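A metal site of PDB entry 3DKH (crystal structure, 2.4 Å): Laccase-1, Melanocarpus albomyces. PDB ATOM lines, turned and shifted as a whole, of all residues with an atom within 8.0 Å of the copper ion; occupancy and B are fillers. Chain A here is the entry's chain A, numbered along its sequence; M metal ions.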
ATOM      1  N   GLU A 235      11.935   4.557 -28.350  1.00  0.00           N
ATOM      2  CA  GLU A 235      12.988   5.086 -27.464  1.00  0.00           C
ATOM      3  C   GLU A 235      12.429   5.989 -26.379  1.00  0.00           C
ATOM      4  O   GLU A 235      12.826   5.875 -25.226  1.00  0.00           O
ATOM      5  CB  GLU A 235      14.067   5.847 -28.257  1.00  0.00           C
ATOM      6  CG  GLU A 235      15.352   6.220 -27.480  1.00  0.00           C
ATOM      7  CD  GLU A 235      15.317   7.575 -26.757  1.00  0.00           C
ATOM      8  OE1 GLU A 235      14.527   8.454 -27.160  1.00  0.00           O
ATOM      9  OE2 GLU A 235      16.065   7.744 -25.779  1.00  0.00           O
ATOM     10  N   HIS A 237      10.612   7.820 -23.391  1.00  0.00           N
ATOM     11  CA  HIS A 237      10.025   7.453 -22.105  1.00  0.00           C
ATOM     12  C   HIS A 237       9.261   8.699 -21.643  1.00  0.00           C
ATOM     13  O   HIS A 237       9.831   9.797 -21.530  1.00  0.00           O
ATOM     14  CB  HIS A 237      11.073   7.111 -21.083  1.00  0.00           C
ATOM     15  CG  HIS A 237      11.935   5.955 -21.454  1.00  0.00           C
ATOM     16  ND1 HIS A 237      12.783   5.975 -22.539  1.00  0.00           N
ATOM     17  CD2 HIS A 237      12.134   4.761 -20.852  1.00  0.00           C
ATOM     18  CE1 HIS A 237      13.470   4.851 -22.576  1.00  0.00           C
ATOM     19  NE2 HIS A 237      13.092   4.098 -21.560  1.00  0.00           N
ATOM     20  N   VAL A 361      25.621  -5.248 -17.946  1.00  0.00           N
ATOM     21  CA  VAL A 361      25.341  -4.536 -19.186  1.00  0.00           C
ATOM     22  C   VAL A 361      26.543  -3.623 -19.424  1.00  0.00           C
ATOM     23  O   VAL A 361      26.938  -2.870 -18.538  1.00  0.00           O
ATOM     24  CB  VAL A 361      24.043  -3.682 -19.072  1.00  0.00           C
ATOM     25  CG1 VAL A 361      23.807  -2.874 -20.335  1.00  0.00           C
ATOM     26  CG2 VAL A 361      22.860  -4.576 -18.800  1.00  0.00           C
ATOM     27  N   TRP A 373      25.915  -2.875 -27.729  1.00  0.00           N
ATOM     28  CA  TRP A 373      25.512  -3.168 -26.349  1.00  0.00           C
ATOM     29  C   TRP A 373      25.720  -4.635 -25.965  1.00  0.00           C
ATOM     30  O   TRP A 373      25.163  -5.524 -26.590  1.00  0.00           O
ATOM     31  CB  TRP A 373      24.058  -2.754 -26.136  1.00  0.00           C
ATOM     32  CG  TRP A 373      23.863  -1.277 -26.181  1.00  0.00           C
ATOM     33  CD1 TRP A 373      23.494  -0.541 -27.266  1.00  0.00           C
ATOM     34  CD2 TRP A 373      24.074  -0.351 -25.117  1.00  0.00           C
ATOM     35  NE1 TRP A 373      23.470   0.794 -26.948  1.00  0.00           N
ATOM     36  CE2 TRP A 373      23.823   0.949 -25.635  1.00  0.00           C
ATOM     37  CE3 TRP A 373      24.460  -0.482 -23.760  1.00  0.00           C
ATOM     38  CZ2 TRP A 373      23.946   2.121 -24.844  1.00  0.00           C
ATOM     39  CZ3 TRP A 373      24.582   0.689 -22.969  1.00  0.00           C
ATOM     40  CH2 TRP A 373      24.326   1.972 -23.524  1.00  0.00           C
ATOM     41  N   ASN A 421      24.314  -1.941 -14.532  1.00  0.00           N
ATOM     42  CA  ASN A 421      24.339  -0.940 -15.614  1.00  0.00           C
ATOM     43  C   ASN A 421      25.667  -0.214 -15.865  1.00  0.00           C
ATOM     44  O   ASN A 421      25.779   0.979 -15.579  1.00  0.00           O
ATOM     45  CB  ASN A 421      23.248   0.106 -15.371  1.00  0.00           C
ATOM     46  CG  ASN A 421      22.789   0.784 -16.649  1.00  0.00           C
ATOM     47  OD1 ASN A 421      23.359   0.600 -17.727  1.00  0.00           O
ATOM     48  ND2 ASN A 421      21.724   1.570 -16.537  1.00  0.00           N
ATOM     49  N   LEU A 429      23.462   5.018 -19.503  1.00  0.00           N
ATOM     50  CA  LEU A 429      22.113   5.459 -19.837  1.00  0.00           C
ATOM     51  C   LEU A 429      21.073   4.556 -19.181  1.00  0.00           C
ATOM     52  O   LEU A 429      21.368   3.392 -18.891  1.00  0.00           O
ATOM     53  CB  LEU A 429      21.941   5.419 -21.369  1.00  0.00           C
ATOM     54  CG  LEU A 429      22.626   6.485 -22.230  1.00  0.00           C
ATOM     55  CD1 LEU A 429      22.590   6.061 -23.694  1.00  0.00           C
ATOM     56  CD2 LEU A 429      21.943   7.834 -22.062  1.00  0.00           C
ATOM     57  N   PRO A 430      19.853   5.083 -18.884  1.00  0.00           N
ATOM     58  CA  PRO A 430      18.788   4.282 -18.262  1.00  0.00           C
ATOM     59  C   PRO A 430      18.236   3.244 -19.258  1.00  0.00           C
ATOM     60  O   PRO A 430      18.152   3.516 -20.466  1.00  0.00           O
ATOM     61  CB  PRO A 430      17.724   5.333 -17.926  1.00  0.00           C
ATOM     62  CG  PRO A 430      18.493   6.573 -17.754  1.00  0.00           C
ATOM     63  CD  PRO A 430      19.451   6.504 -18.912  1.00  0.00           C
ATOM     64  N   HIS A 431      17.906   2.047 -18.761  1.00  0.00           N
ATOM     65  CA  HIS A 431      17.410   0.975 -19.631  1.00  0.00           C
ATOM     66  C   HIS A 431      16.091   0.334 -19.200  1.00  0.00           C
ATOM     67  O   HIS A 431      16.018  -0.233 -18.117  1.00  0.00           O
ATOM     68  CB  HIS A 431      18.460  -0.151 -19.792  1.00  0.00           C
ATOM     69  CG  HIS A 431      19.758   0.288 -20.420  1.00  0.00           C
ATOM     70  ND1 HIS A 431      19.816   0.993 -21.593  1.00  0.00           N
ATOM     71  CD2 HIS A 431      21.038   0.111 -20.019  1.00  0.00           C
ATOM     72  CE1 HIS A 431      21.080   1.238 -21.894  1.00  0.00           C
ATOM     73  NE2 HIS A 431      21.843   0.710 -20.956  1.00  0.00           N
ATOM     74  N   PRO A 432      15.026   0.434 -20.027  1.00  0.00           N
ATOM     75  CA  PRO A 432      13.734  -0.175 -19.713  1.00  0.00           C
ATOM     76  C   PRO A 432      13.807  -1.686 -19.953  1.00  0.00           C
ATOM     77  O   PRO A 432      13.677  -2.156 -21.077  1.00  0.00           O
ATOM     78  CB  PRO A 432      12.786   0.541 -20.676  1.00  0.00           C
ATOM     79  CG  PRO A 432      13.652   0.829 -21.860  1.00  0.00           C
ATOM     80  CD  PRO A 432      14.911   1.315 -21.211  1.00  0.00           C
ATOM     81  N   MET A 433      14.151  -2.422 -18.915  1.00  0.00           N
ATOM     82  CA  MET A 433      14.273  -3.874 -19.017  1.00  0.00           C
ATOM     83  C   MET A 433      12.929  -4.588 -19.064  1.00  0.00           C
ATOM     84  O   MET A 433      12.049  -4.370 -18.237  1.00  0.00           O
ATOM     85  CB  MET A 433      15.158  -4.419 -17.900  1.00  0.00           C
ATOM     86  CG  MET A 433      16.597  -3.920 -17.965  1.00  0.00           C
ATOM     87  SD  MET A 433      17.399  -4.038 -19.578  1.00  0.00           S
ATOM     88  CE  MET A 433      18.015  -5.678 -19.556  1.00  0.00           C
ATOM     89  N   MET A 480      12.598  -0.054 -15.047  1.00  0.00           N
ATOM     90  CA  MET A 480      13.840   0.654 -15.335  1.00  0.00           C
ATOM     91  C   MET A 480      15.104   0.173 -14.652  1.00  0.00           C
ATOM     92  O   MET A 480      15.135  -0.044 -13.443  1.00  0.00           O
ATOM     93  CB  MET A 480      13.699   2.149 -15.048  1.00  0.00           C
ATOM     94  CG  MET A 480      12.725   2.889 -15.941  1.00  0.00           C
ATOM     95  SD  MET A 480      13.049   2.664 -17.677  1.00  0.00           S
ATOM     96  CE  MET A 480      14.450   3.713 -17.902  1.00  0.00           C
ATOM     97  N   LEU A 481      16.157   0.009 -15.454  1.00  0.00           N
ATOM     98  CA  LEU A 481      17.475  -0.327 -14.943  1.00  0.00           C
ATOM     99  C   LEU A 481      18.075   1.076 -14.907  1.00  0.00           C
ATOM    100  O   LEU A 481      18.254   1.721 -15.949  1.00  0.00           O
ATOM    101  CB  LEU A 481      18.235  -1.252 -15.895  1.00  0.00           C
ATOM    102  CG  LEU A 481      19.748  -1.462 -15.768  1.00  0.00           C
ATOM    103  CD1 LEU A 481      20.154  -2.113 -14.477  1.00  0.00           C
ATOM    104  CD2 LEU A 481      20.253  -2.260 -16.944  1.00  0.00           C
ATOM    105  N   HIS A 502      15.340  -8.264 -22.577  1.00  0.00           N
ATOM    106  CA  HIS A 502      16.032  -7.202 -23.244  1.00  0.00           C
ATOM    107  C   HIS A 502      15.591  -5.799 -22.895  1.00  0.00           C
ATOM    108  O   HIS A 502      14.533  -5.593 -22.285  1.00  0.00           O
ATOM    109  CB  HIS A 502      15.888  -7.393 -24.771  1.00  0.00           C
ATOM    110  CG  HIS A 502      14.501  -7.181 -25.295  1.00  0.00           C
ATOM    111  ND1 HIS A 502      14.103  -5.999 -25.877  1.00  0.00           N
ATOM    112  CD2 HIS A 502      13.419  -8.002 -25.310  1.00  0.00           C
ATOM    113  CE1 HIS A 502      12.835  -6.092 -26.244  1.00  0.00           C
ATOM    114  NE2 HIS A 502      12.398  -7.301 -25.908  1.00  0.00           N
ATOM    115  N   CYS A 503      16.389  -4.845 -23.367  1.00  0.00           N
ATOM    116  CA  CYS A 503      16.095  -3.431 -23.208  1.00  0.00           C
ATOM    117  C   CYS A 503      15.089  -3.188 -24.320  1.00  0.00           C
ATOM    118  O   CYS A 503      15.263  -3.679 -25.449  1.00  0.00           O
ATOM    119  CB  CYS A 503      17.333  -2.582 -23.468  1.00  0.00           C
ATOM    120  SG  CYS A 503      16.938  -0.841 -23.440  1.00  0.00           S
ATOM    121  N   HIS A 504      14.021  -2.452 -23.994  1.00  0.00           N
ATOM    122  CA  HIS A 504      12.999  -2.174 -24.980  1.00  0.00           C
ATOM    123  C   HIS A 504      13.214  -0.948 -25.884  1.00  0.00           C
ATOM    124  O   HIS A 504      12.379  -0.655 -26.741  1.00  0.00           O
ATOM    125  CB  HIS A 504      11.616  -2.225 -24.358  1.00  0.00           C
ATOM    126  CG  HIS A 504      10.571  -2.769 -25.284  1.00  0.00           C
ATOM    127  ND1 HIS A 504      10.202  -2.125 -26.446  1.00  0.00           N
ATOM    128  CD2 HIS A 504       9.854  -3.910 -25.239  1.00  0.00           C
ATOM    129  CE1 HIS A 504       9.298  -2.841 -27.077  1.00  0.00           C
ATOM    130  NE2 HIS A 504       9.069  -3.929 -26.362  1.00  0.00           N
ATOM    131  N   ILE A 505      14.325  -0.225 -25.680  1.00  0.00           N
ATOM    132  CA  ILE A 505      14.679   0.890 -26.574  1.00  0.00           C
ATOM    133  C   ILE A 505      15.128   0.107 -27.827  1.00  0.00           C
ATOM    134  O   ILE A 505      16.027  -0.740 -27.739  1.00  0.00           O
ATOM    135  CB  ILE A 505      15.851   1.767 -26.039  1.00  0.00           C
ATOM    136  CG1 ILE A 505      15.347   2.702 -24.947  1.00  0.00           C
ATOM    137  CG2 ILE A 505      16.504   2.588 -27.184  1.00  0.00           C
ATOM    138  CD1 ILE A 505      16.437   3.374 -24.109  1.00  0.00           C
ATOM    139  N   ALA A 506      14.392   0.303 -28.922  1.00  0.00           N
ATOM    140  CA  ALA A 506      14.619  -0.379 -30.198  1.00  0.00           C
ATOM    141  C   ALA A 506      16.053  -0.387 -30.669  1.00  0.00           C
ATOM    142  O   ALA A 506      16.583  -1.436 -31.030  1.00  0.00           O
ATOM    143  CB  ALA A 506      13.734   0.186 -31.265  1.00  0.00           C
ATOM    144  N   TRP A 507      16.698   0.765 -30.536  1.00  0.00           N
ATOM    145  CA  TRP A 507      18.088   0.950 -30.949  1.00  0.00           C
ATOM    146  C   TRP A 507      19.078   0.153 -30.103  1.00  0.00           C
ATOM    147  O   TRP A 507      20.080  -0.366 -30.619  1.00  0.00           O
ATOM    148  CB  TRP A 507      18.464   2.430 -30.933  1.00  0.00           C
ATOM    149  CG  TRP A 507      17.346   3.461 -31.203  1.00  0.00           C
ATOM    150  CD1 TRP A 507      17.142   4.604 -30.484  1.00  0.00           C
ATOM    151  CD2 TRP A 507      16.311   3.446 -32.221  1.00  0.00           C
ATOM    152  NE1 TRP A 507      16.072   5.304 -30.970  1.00  0.00           N
ATOM    153  CE2 TRP A 507      15.530   4.625 -32.029  1.00  0.00           C
ATOM    154  CE3 TRP A 507      15.971   2.555 -33.269  1.00  0.00           C
ATOM    155  CZ2 TRP A 507      14.415   4.930 -32.849  1.00  0.00           C
ATOM    156  CZ3 TRP A 507      14.859   2.857 -34.079  1.00  0.00           C
ATOM    157  CH2 TRP A 507      14.088   4.050 -33.863  1.00  0.00           C
ATOM    158  N   HIS A 508      18.767   0.003 -28.818  1.00  0.00           N
ATOM    159  CA  HIS A 508      19.616  -0.733 -27.889  1.00  0.00           C
ATOM    160  C   HIS A 508      19.551  -2.250 -28.027  1.00  0.00           C
ATOM    161  O   HIS A 508      20.601  -2.918 -27.974  1.00  0.00           O
ATOM    162  CB  HIS A 508      19.377  -0.268 -26.444  1.00  0.00           C
ATOM    163  CG  HIS A 508      19.761   1.163 -26.195  1.00  0.00           C
ATOM    164  ND1 HIS A 508      19.483   1.807 -25.016  1.00  0.00           N
ATOM    165  CD2 HIS A 508      20.397   2.066 -26.979  1.00  0.00           C
ATOM    166  CE1 HIS A 508      19.928   3.051 -25.080  1.00  0.00           C
ATOM    167  NE2 HIS A 508      20.491   3.231 -26.260  1.00  0.00           N
ATOM    168  N   VAL A 509      18.362  -2.793 -28.266  1.00  0.00           N
ATOM    169  CA  VAL A 509      18.189  -4.243 -28.471  1.00  0.00           C
ATOM    170  C   VAL A 509      18.813  -4.613 -29.827  1.00  0.00           C
ATOM    171  O   VAL A 509      19.335  -5.719 -29.997  1.00  0.00           O
ATOM    172  CB  VAL A 509      16.692  -4.721 -28.317  1.00  0.00           C
ATOM    173  CG1 VAL A 509      15.781  -4.101 -29.357  1.00  0.00           C
ATOM    174  CG2 VAL A 509      16.613  -6.240 -28.353  1.00  0.00           C
ATOM    175  N   LEU A 513      21.634  -5.419 -26.681  1.00  0.00           N
ATOM    176  CA  LEU A 513      21.187  -5.500 -25.292  1.00  0.00           C
ATOM    177  C   LEU A 513      20.053  -6.489 -25.077  1.00  0.00           C
ATOM    178  O   LEU A 513      18.876  -6.097 -24.994  1.00  0.00           O
ATOM    179  CB  LEU A 513      20.801  -4.127 -24.748  1.00  0.00           C
ATOM    180  CG  LEU A 513      21.352  -3.753 -23.359  1.00  0.00           C
ATOM    181  CD1 LEU A 513      21.316  -2.256 -23.233  1.00  0.00           C
ATOM    182  CD2 LEU A 513      20.580  -4.415 -22.223  1.00  0.00           C
HETATM  183 CU    CU M   1      18.732   0.411 -23.375  1.00  0.00          CU
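The backbone carbonyl oxygen of Leu 429 sits at hydrogen-bond distance from a ring nitrogen (NE2) of His 431 (3.4 Å).
O of His 431 lies within hydrogen-bond range of N of Leu 481, at 2.7 Å.
The backbone NH of Cys 503 is in hydrogen-bond range of the backbone carbonyl oxygen of Leu 513 (3.2 Å).
N of Ile 505 sits close to SG of Cys 503.
O of His 508 sits at hydrogen-bond distance from N of Leu 513 (3.0 Å).
The copper ion is bound by ND1 of His 431 (2.2 Å), SG of Cys 503 (2.2 Å) and ND1 of His 508 (2.3 Å).
The copper ion has three donor atoms within binding distance.
Residues that only touch the copper ion: Leu 513 (3.7 Å) and Ile 505 (3.8 Å).
Of the 21 residues printed, 5 come within 4 Å of the copper ion.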
